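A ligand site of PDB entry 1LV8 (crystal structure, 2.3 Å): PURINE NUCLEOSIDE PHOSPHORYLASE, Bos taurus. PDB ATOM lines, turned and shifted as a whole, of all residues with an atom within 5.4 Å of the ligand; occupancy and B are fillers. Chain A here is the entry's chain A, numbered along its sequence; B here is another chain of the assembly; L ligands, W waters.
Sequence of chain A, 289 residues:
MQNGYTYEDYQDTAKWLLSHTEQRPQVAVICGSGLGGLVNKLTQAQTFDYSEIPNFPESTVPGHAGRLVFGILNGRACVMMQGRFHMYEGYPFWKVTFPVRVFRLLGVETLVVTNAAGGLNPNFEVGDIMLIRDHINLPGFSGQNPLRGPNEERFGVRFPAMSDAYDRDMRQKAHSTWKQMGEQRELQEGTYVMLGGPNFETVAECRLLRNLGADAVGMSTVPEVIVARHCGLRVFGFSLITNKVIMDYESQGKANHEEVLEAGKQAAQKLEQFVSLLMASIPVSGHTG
The backbone NH (N) of Gly 118 sits at hydrogen-bond distance from a nitrogen (N2) of the ligand (3.4 Å).
NE2 of His 86 lies close to O4 of the ligand.
ND2 of Asn 243 lies within hydrogen-bond range of N2 of the ligand (2.9 Å).
The side-chain hydroxyl (OG) of Ser 220 lies within hydrogen-bond range of an oxygen (O3) of the ligand (2.6 Å).
N of Ser 33 sits at hydrogen-bond distance from O2 of the ligand (2.9 Å).
N of Ala 116 sits at hydrogen-bond distance from O2 of the ligand.
OE2 of Glu 201 sits at hydrogen-bond distance from N5 of the ligand, at 2.5 Å.
The backbone NH (N) of Gly 118 is in hydrogen-bond range of the backbone carbonyl oxygen (O) of Val 217 (2.9 Å).
N of Ser 220 is in hydrogen-bond range of OH of Tyr 192, at 3.2 Å.
The backbone NH (N) of Gly 32 sits close to the backbone carbonyl oxygen (O) of Thr 114, at 3.3 Å.
The backbone NH (N) of Met 219 lies within hydrogen-bond range of the side-chain hydroxyl (OH) of Tyr 192.
O of Thr 114 is in hydrogen-bond range of NH2 of Arg 84, at 2.8 Å.
The side-chain hydroxyl (OG) of Ser 220 sits at hydrogen-bond distance from the side-chain hydroxyl (OG1) of Thr 221 (3.0 Å).
O of Gly 218 lies within hydrogen-bond range of N of Leu 195, at 3.0 Å.
The guanidinium group (NH2) of Arg 84 lies within hydrogen-bond range of the side-chain hydroxyl (OG1) of Thr 221.
Merely in contact with the ligand: Gly 32, Arg 84, Asn 115, Ala 117, Leu 195, Phe 200, Val 217, Gly 218, Met 219 and Phe 159 of chain B.
Water W1 lies within hydrogen-bond range of an oxygen (O3) of the ligand (2.5 Å), the backbone NH (N) of Met 219 (3.0 Å), a ring nitrogen (ND1) of His 86 (3.5 Å) and the backbone NH (N) of Ser 220 (3.5 Å).
Water W3 bridges OE1 of Glu 201 (2.7 Å) and N3 of the ligand (2.8 Å).
Water W2 lies within hydrogen-bond range of the side-chain hydroxyl of Tyr 192, the backbone carbonyl oxygen of Ala 116, an oxygen (O3) of the ligand and the backbone NH of Met 219.
Water W4 lies within hydrogen-bond range of N of Ser 33 (3.1 Å) and O4 of the ligand (3.2 Å).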
ATOM      1  N   GLY A  32      29.694 -37.309  -9.841  1.00  0.00           N
ATOM      2  CA  GLY A  32      28.907 -36.200  -9.351  1.00  0.00           C
ATOM      3  C   GLY A  32      27.828 -36.659  -8.387  1.00  0.00           C
ATOM      4  O   GLY A  32      27.716 -37.852  -8.083  1.00  0.00           O
ATOM      5  N   SER A  33      27.038 -35.708  -7.903  1.00  0.00           N
ATOM      6  CA  SER A  33      25.948 -36.001  -6.972  1.00  0.00           C
ATOM      7  C   SER A  33      25.057 -37.160  -7.416  1.00  0.00           C
ATOM      8  O   SER A  33      24.483 -37.144  -8.515  1.00  0.00           O
ATOM      9  CB  SER A  33      25.089 -34.745  -6.754  1.00  0.00           C
ATOM     10  OG  SER A  33      23.835 -35.077  -6.175  1.00  0.00           O
ATOM     11  N   ARG A  84      32.993 -35.255  -4.435  1.00  0.00           N
ATOM     12  CA  ARG A  84      33.901 -34.268  -5.011  1.00  0.00           C
ATOM     13  C   ARG A  84      33.791 -32.986  -4.193  1.00  0.00           C
ATOM     14  O   ARG A  84      32.948 -32.911  -3.284  1.00  0.00           O
ATOM     15  CB  ARG A  84      33.504 -33.997  -6.455  1.00  0.00           C
ATOM     16  CG  ARG A  84      32.034 -33.656  -6.621  1.00  0.00           C
ATOM     17  CD  ARG A  84      31.806 -32.689  -7.797  1.00  0.00           C
ATOM     18  NE  ARG A  84      31.748 -33.365  -9.093  1.00  0.00           N
ATOM     19  CZ  ARG A  84      32.274 -32.853 -10.193  1.00  0.00           C
ATOM     20  NH1 ARG A  84      32.875 -31.670 -10.132  1.00  0.00           N
ATOM     21  NH2 ARG A  84      32.209 -33.506 -11.349  1.00  0.00           N
ATOM     22  N   HIS A  86      33.331 -28.564  -3.901  1.00  0.00           N
ATOM     23  CA  HIS A  86      32.671 -27.424  -4.549  1.00  0.00           C
ATOM     24  C   HIS A  86      33.045 -26.060  -4.003  1.00  0.00           C
ATOM     25  O   HIS A  86      33.295 -25.900  -2.840  1.00  0.00           O
ATOM     26  CB  HIS A  86      31.144 -27.502  -4.402  1.00  0.00           C
ATOM     27  CG  HIS A  86      30.553 -28.813  -4.793  1.00  0.00           C
ATOM     28  ND1 HIS A  86      29.902 -29.001  -5.995  1.00  0.00           N
ATOM     29  CD2 HIS A  86      30.518 -29.997  -4.152  1.00  0.00           C
ATOM     30  CE1 HIS A  86      29.495 -30.252  -6.073  1.00  0.00           C
ATOM     31  NE2 HIS A  86      29.859 -30.880  -4.965  1.00  0.00           N
ATOM     32  N   TYR A  88      30.987 -23.695  -3.581  1.00  0.00           N
ATOM     33  CA  TYR A  88      29.961 -23.239  -2.649  1.00  0.00           C
ATOM     34  C   TYR A  88      30.126 -23.747  -1.201  1.00  0.00           C
ATOM     35  O   TYR A  88      29.499 -23.216  -0.276  1.00  0.00           O
ATOM     36  CB  TYR A  88      28.566 -23.585  -3.180  1.00  0.00           C
ATOM     37  CG  TYR A  88      28.213 -25.061  -3.184  1.00  0.00           C
ATOM     38  CD1 TYR A  88      28.117 -25.797  -1.992  1.00  0.00           C
ATOM     39  CD2 TYR A  88      27.996 -25.742  -4.394  1.00  0.00           C
ATOM     40  CE1 TYR A  88      27.817 -27.151  -1.990  1.00  0.00           C
ATOM     41  CE2 TYR A  88      27.699 -27.101  -4.420  1.00  0.00           C
ATOM     42  CZ  TYR A  88      27.604 -27.793  -3.214  1.00  0.00           C
ATOM     43  OH  TYR A  88      27.285 -29.119  -3.271  1.00  0.00           O
ATOM     44  N   THR A 114      31.742 -36.416 -14.329  1.00  0.00           N
ATOM     45  CA  THR A 114      30.309 -36.553 -14.397  1.00  0.00           C
ATOM     46  C   THR A 114      29.686 -35.640 -13.371  1.00  0.00           C
ATOM     47  O   THR A 114      30.333 -35.318 -12.393  1.00  0.00           O
ATOM     48  CB  THR A 114      29.842 -38.022 -14.077  1.00  0.00           C
ATOM     49  OG1 THR A 114      28.487 -38.170 -14.481  1.00  0.00           O
ATOM     50  CG2 THR A 114      29.887 -38.306 -12.559  1.00  0.00           C
ATOM     51  N   ASN A 115      28.437 -35.222 -13.579  1.00  0.00           N
ATOM     52  CA  ASN A 115      27.792 -34.392 -12.591  1.00  0.00           C
ATOM     53  C   ASN A 115      26.290 -34.385 -12.799  1.00  0.00           C
ATOM     54  O   ASN A 115      25.807 -34.837 -13.837  1.00  0.00           O
ATOM     55  CB  ASN A 115      28.339 -32.953 -12.675  1.00  0.00           C
ATOM     56  CG  ASN A 115      28.026 -32.282 -14.024  1.00  0.00           C
ATOM     57  OD1 ASN A 115      28.923 -31.712 -14.673  1.00  0.00           O
ATOM     58  ND2 ASN A 115      26.765 -32.333 -14.440  1.00  0.00           N
ATOM     59  N   ALA A 116      25.539 -33.876 -11.837  1.00  0.00           N
ATOM     60  CA  ALA A 116      24.082 -33.794 -12.024  1.00  0.00           C
ATOM     61  C   ALA A 116      23.805 -32.323 -12.337  1.00  0.00           C
ATOM     62  O   ALA A 116      24.444 -31.453 -11.780  1.00  0.00           O
ATOM     63  CB  ALA A 116      23.377 -34.209 -10.758  1.00  0.00           C
ATOM     64  N   ALA A 117      22.854 -32.027 -13.198  1.00  0.00           N
ATOM     65  CA  ALA A 117      22.621 -30.635 -13.533  1.00  0.00           C
ATOM     66  C   ALA A 117      21.177 -30.251 -13.850  1.00  0.00           C
ATOM     67  O   ALA A 117      20.296 -31.086 -14.079  1.00  0.00           O
ATOM     68  CB  ALA A 117      23.533 -30.252 -14.689  1.00  0.00           C
ATOM     69  N   GLY A 118      20.945 -28.944 -13.848  1.00  0.00           N
ATOM     70  CA  GLY A 118      19.628 -28.426 -14.150  1.00  0.00           C
ATOM     71  C   GLY A 118      19.557 -28.268 -15.655  1.00  0.00           C
ATOM     72  O   GLY A 118      20.569 -27.909 -16.297  1.00  0.00           O
ATOM     73  N   TYR A 192      27.719 -26.855 -20.945  1.00  0.00           N
ATOM     74  CA  TYR A 192      27.537 -26.802 -19.498  1.00  0.00           C
ATOM     75  C   TYR A 192      28.077 -25.471 -18.935  1.00  0.00           C
ATOM     76  O   TYR A 192      29.229 -25.100 -19.173  1.00  0.00           O
ATOM     77  CB  TYR A 192      28.271 -27.993 -18.844  1.00  0.00           C
ATOM     78  CG  TYR A 192      28.214 -27.995 -17.316  1.00  0.00           C
ATOM     79  CD1 TYR A 192      29.145 -27.262 -16.565  1.00  0.00           C
ATOM     80  CD2 TYR A 192      27.267 -28.753 -16.616  1.00  0.00           C
ATOM     81  CE1 TYR A 192      29.145 -27.272 -15.187  1.00  0.00           C
ATOM     82  CE2 TYR A 192      27.260 -28.779 -15.221  1.00  0.00           C
ATOM     83  CZ  TYR A 192      28.208 -28.036 -14.506  1.00  0.00           C
ATOM     84  OH  TYR A 192      28.282 -28.121 -13.146  1.00  0.00           O
ATOM     85  N   LEU A 195      28.236 -22.071 -12.362  1.00  0.00           N
ATOM     86  CA  LEU A 195      28.127 -20.855 -11.560  1.00  0.00           C
ATOM     87  C   LEU A 195      28.346 -21.306 -10.122  1.00  0.00           C
ATOM     88  O   LEU A 195      28.372 -22.520  -9.830  1.00  0.00           O
ATOM     89  CB  LEU A 195      26.792 -20.113 -11.741  1.00  0.00           C
ATOM     90  CG  LEU A 195      25.515 -20.848 -12.055  1.00  0.00           C
ATOM     91  CD1 LEU A 195      25.131 -21.625 -10.773  1.00  0.00           C
ATOM     92  CD2 LEU A 195      24.422 -19.820 -12.453  1.00  0.00           C
ATOM     93  N   ASN A 199      22.527 -21.496  -3.873  1.00  0.00           N
ATOM     94  CA  ASN A 199      21.103 -21.334  -4.093  1.00  0.00           C
ATOM     95  C   ASN A 199      20.812 -21.704  -5.541  1.00  0.00           C
ATOM     96  O   ASN A 199      21.706 -21.654  -6.359  1.00  0.00           O
ATOM     97  CB  ASN A 199      20.651 -19.885  -3.846  1.00  0.00           C
ATOM     98  CG  ASN A 199      21.231 -18.893  -4.864  1.00  0.00           C
ATOM     99  OD1 ASN A 199      20.615 -18.581  -5.896  1.00  0.00           O
ATOM    100  ND2 ASN A 199      22.405 -18.405  -4.575  1.00  0.00           N
ATOM    101  N   PHE A 200      19.570 -22.073  -5.863  1.00  0.00           N
ATOM    102  CA  PHE A 200      19.250 -22.394  -7.253  1.00  0.00           C
ATOM    103  C   PHE A 200      18.828 -21.107  -7.937  1.00  0.00           C
ATOM    104  O   PHE A 200      18.524 -20.131  -7.278  1.00  0.00           O
ATOM    105  CB  PHE A 200      18.170 -23.505  -7.319  1.00  0.00           C
ATOM    106  CG  PHE A 200      18.747 -24.907  -7.236  1.00  0.00           C
ATOM    107  CD1 PHE A 200      19.996 -25.134  -6.666  1.00  0.00           C
ATOM    108  CD2 PHE A 200      18.065 -25.996  -7.787  1.00  0.00           C
ATOM    109  CE1 PHE A 200      20.572 -26.408  -6.638  1.00  0.00           C
ATOM    110  CE2 PHE A 200      18.625 -27.276  -7.760  1.00  0.00           C
ATOM    111  CZ  PHE A 200      19.879 -27.483  -7.193  1.00  0.00           C
ATOM    112  N   GLU A 201      18.814 -21.106  -9.257  1.00  0.00           N
ATOM    113  CA  GLU A 201      18.540 -19.896 -10.036  1.00  0.00           C
ATOM    114  C   GLU A 201      17.194 -19.227  -9.957  1.00  0.00           C
ATOM    115  O   GLU A 201      16.184 -19.852  -9.671  1.00  0.00           O
ATOM    116  CB  GLU A 201      18.828 -20.174 -11.519  1.00  0.00           C
ATOM    117  CG  GLU A 201      20.283 -20.498 -11.817  1.00  0.00           C
ATOM    118  CD  GLU A 201      20.725 -21.831 -11.258  1.00  0.00           C
ATOM    119  OE1 GLU A 201      19.968 -22.808 -11.361  1.00  0.00           O
ATOM    120  OE2 GLU A 201      21.861 -21.896 -10.736  1.00  0.00           O
ATOM    121  N   VAL A 217      22.971 -26.188 -16.308  1.00  0.00           N
ATOM    122  CA  VAL A 217      23.679 -25.412 -15.278  1.00  0.00           C
ATOM    123  C   VAL A 217      24.029 -26.277 -14.097  1.00  0.00           C
ATOM    124  O   VAL A 217      23.229 -27.123 -13.700  1.00  0.00           O
ATOM    125  CB  VAL A 217      22.827 -24.312 -14.621  1.00  0.00           C
ATOM    126  CG1 VAL A 217      23.004 -23.032 -15.333  1.00  0.00           C
ATOM    127  CG2 VAL A 217      21.367 -24.729 -14.572  1.00  0.00           C
ATOM    128  N   GLY A 218      25.193 -26.003 -13.505  1.00  0.00           N
ATOM    129  CA  GLY A 218      25.637 -26.726 -12.323  1.00  0.00           C
ATOM    130  C   GLY A 218      26.675 -25.919 -11.571  1.00  0.00           C
ATOM    131  O   GLY A 218      27.048 -24.819 -12.000  1.00  0.00           O
ATOM    132  N   MET A 219      27.187 -26.475 -10.477  1.00  0.00           N
ATOM    133  CA  MET A 219      28.155 -25.774  -9.656  1.00  0.00           C
ATOM    134  C   MET A 219      29.483 -26.482  -9.541  1.00  0.00           C
ATOM    135  O   MET A 219      30.133 -26.431  -8.480  1.00  0.00           O
ATOM    136  CB  MET A 219      27.573 -25.552  -8.264  1.00  0.00           C
ATOM    137  CG  MET A 219      26.097 -25.117  -8.239  1.00  0.00           C
ATOM    138  SD  MET A 219      25.383 -25.192  -6.560  1.00  0.00           S
ATOM    139  CE  MET A 219      23.716 -24.730  -6.852  1.00  0.00           C
ATOM    140  N   SER A 220      29.911 -27.147 -10.615  1.00  0.00           N
ATOM    141  CA  SER A 220      31.205 -27.840 -10.536  1.00  0.00           C
ATOM    142  C   SER A 220      31.795 -28.154 -11.902  1.00  0.00           C
ATOM    143  O   SER A 220      31.435 -27.543 -12.904  1.00  0.00           O
ATOM    144  CB  SER A 220      31.034 -29.159  -9.794  1.00  0.00           C
ATOM    145  OG  SER A 220      30.257 -30.060 -10.599  1.00  0.00           O
ATOM    146  N   THR A 221      32.742 -29.097 -11.899  1.00  0.00           N
ATOM    147  CA  THR A 221      33.327 -29.658 -13.101  1.00  0.00           C
ATOM    148  C   THR A 221      34.257 -28.797 -13.918  1.00  0.00           C
ATOM    149  O   THR A 221      35.384 -29.206 -14.211  1.00  0.00           O
ATOM    150  CB  THR A 221      32.178 -30.193 -13.995  1.00  0.00           C
ATOM    151  OG1 THR A 221      31.357 -31.044 -13.193  1.00  0.00           O
ATOM    152  CG2 THR A 221      32.719 -30.965 -15.214  1.00  0.00           C
ATOM    153  N   THR A 242      18.970 -34.033 -13.764  1.00  0.00           N
ATOM    154  CA  THR A 242      18.065 -34.451 -12.687  1.00  0.00           C
ATOM    155  C   THR A 242      16.889 -33.504 -12.470  1.00  0.00           C
ATOM    156  O   THR A 242      16.022 -33.749 -11.633  1.00  0.00           O
ATOM    157  CB  THR A 242      18.792 -34.584 -11.309  1.00  0.00           C
ATOM    158  OG1 THR A 242      19.209 -33.299 -10.858  1.00  0.00           O
ATOM    159  CG2 THR A 242      19.992 -35.500 -11.420  1.00  0.00           C
ATOM    160  N   ASN A 243      16.859 -32.410 -13.205  1.00  0.00           N
ATOM    161  CA  ASN A 243      15.743 -31.486 -13.018  1.00  0.00           C
ATOM    162  C   ASN A 243      15.703 -30.442 -14.102  1.00  0.00           C
ATOM    163  O   ASN A 243      16.717 -30.168 -14.748  1.00  0.00           O
ATOM    164  CB  ASN A 243      15.811 -30.819 -11.632  1.00  0.00           C
ATOM    165  CG  ASN A 243      17.054 -29.956 -11.435  1.00  0.00           C
ATOM    166  OD1 ASN A 243      16.984 -28.710 -11.463  1.00  0.00           O
ATOM    167  ND2 ASN A 243      18.188 -30.607 -11.243  1.00  0.00           N
ATOM    168  N   VAL A 245      14.918 -26.550 -14.926  1.00  0.00           N
ATOM    169  CA  VAL A 245      14.815 -25.285 -14.199  1.00  0.00           C
ATOM    170  C   VAL A 245      13.534 -24.521 -14.478  1.00  0.00           C
ATOM    171  O   VAL A 245      12.920 -24.686 -15.534  1.00  0.00           O
ATOM    172  CB  VAL A 245      16.046 -24.402 -14.517  1.00  0.00           C
ATOM    173  CG1 VAL A 245      17.275 -25.304 -14.684  1.00  0.00           C
ATOM    174  CG2 VAL A 245      15.798 -23.546 -15.769  1.00  0.00           C
ATOM    175  N   PHE B 159      20.555 -26.016  -0.617  1.00  0.00           N
ATOM    176  CA  PHE B 159      20.346 -25.433  -1.934  1.00  0.00           C
ATOM    177  C   PHE B 159      18.983 -24.744  -1.963  1.00  0.00           C
ATOM    178  O   PHE B 159      18.038 -25.258  -2.548  1.00  0.00           O
ATOM    179  CB  PHE B 159      20.345 -26.533  -3.008  1.00  0.00           C
ATOM    180  CG  PHE B 159      21.564 -27.413  -2.984  1.00  0.00           C
ATOM    181  CD1 PHE B 159      22.819 -26.920  -3.397  1.00  0.00           C
ATOM    182  CD2 PHE B 159      21.474 -28.738  -2.542  1.00  0.00           C
ATOM    183  CE1 PHE B 159      23.964 -27.748  -3.380  1.00  0.00           C
ATOM    184  CE2 PHE B 159      22.589 -29.589  -2.517  1.00  0.00           C
ATOM    185  CZ  PHE B 159      23.871 -29.083  -2.937  1.00  0.00           C
HETATM  186  N1  LIG L   1      22.709 -28.915  -9.830  1.00  0.00           N
HETATM  187  C1  LIG L   1      21.629 -29.779 -10.068  1.00  0.00           C
HETATM  188  N2  LIG L   1      20.549 -29.087 -10.442  1.00  0.00           N
HETATM  189  C2  LIG L   1      20.906 -27.730 -10.458  1.00  0.00           C
HETATM  190  C3  LIG L   1      20.157 -26.496 -10.795  1.00  0.00           C
HETATM  191  N3  LIG L   1      18.957 -26.408 -11.149  1.00  0.00           N
HETATM  192  N4  LIG L   1      20.949 -25.305 -10.671  1.00  0.00           N
HETATM  193  C4  LIG L   1      22.308 -25.295 -10.276  1.00  0.00           C
HETATM  194  N5  LIG L   1      22.939 -24.109 -10.211  1.00  0.00           N
HETATM  195  N6  LIG L   1      23.000 -26.442  -9.957  1.00  0.00           N
HETATM  196  C5  LIG L   1      22.265 -27.606 -10.071  1.00  0.00           C
HETATM  197  C6  LIG L   1      24.018 -29.249  -9.441  1.00  0.00           C
HETATM  198  C7  LIG L   1      24.156 -30.009  -8.108  1.00  0.00           C
HETATM  199  C8  LIG L   1      23.830 -29.018  -6.981  1.00  0.00           C
HETATM  200  O1  LIG L   1      25.536 -30.472  -7.945  1.00  0.00           O
HETATM  201  P1  LIG L   1      27.313 -32.055  -8.794  1.00  0.00           P
HETATM  202  C9  LIG L   1      25.798 -31.769  -8.578  1.00  0.00           C
HETATM  203  O2  LIG L   1      27.491 -33.322  -9.525  1.00  0.00           O
HETATM  204  O3  LIG L   1      27.975 -30.973  -9.621  1.00  0.00           O
HETATM  205  O4  LIG L   1      28.024 -32.112  -7.499  1.00  0.00           O
HETATM  206  O   HOH W   1      27.572 -28.697  -8.553  1.00  0.00           O
HETATM  207  O   HOH W   2      26.558 -29.550 -11.753  1.00  0.00           O
HETATM  208  O   HOH W   3      17.572 -23.957 -11.242  1.00  0.00           O
HETATM  209  O   HOH W   4      28.671 -34.484  -5.521  1.00  0.00           O
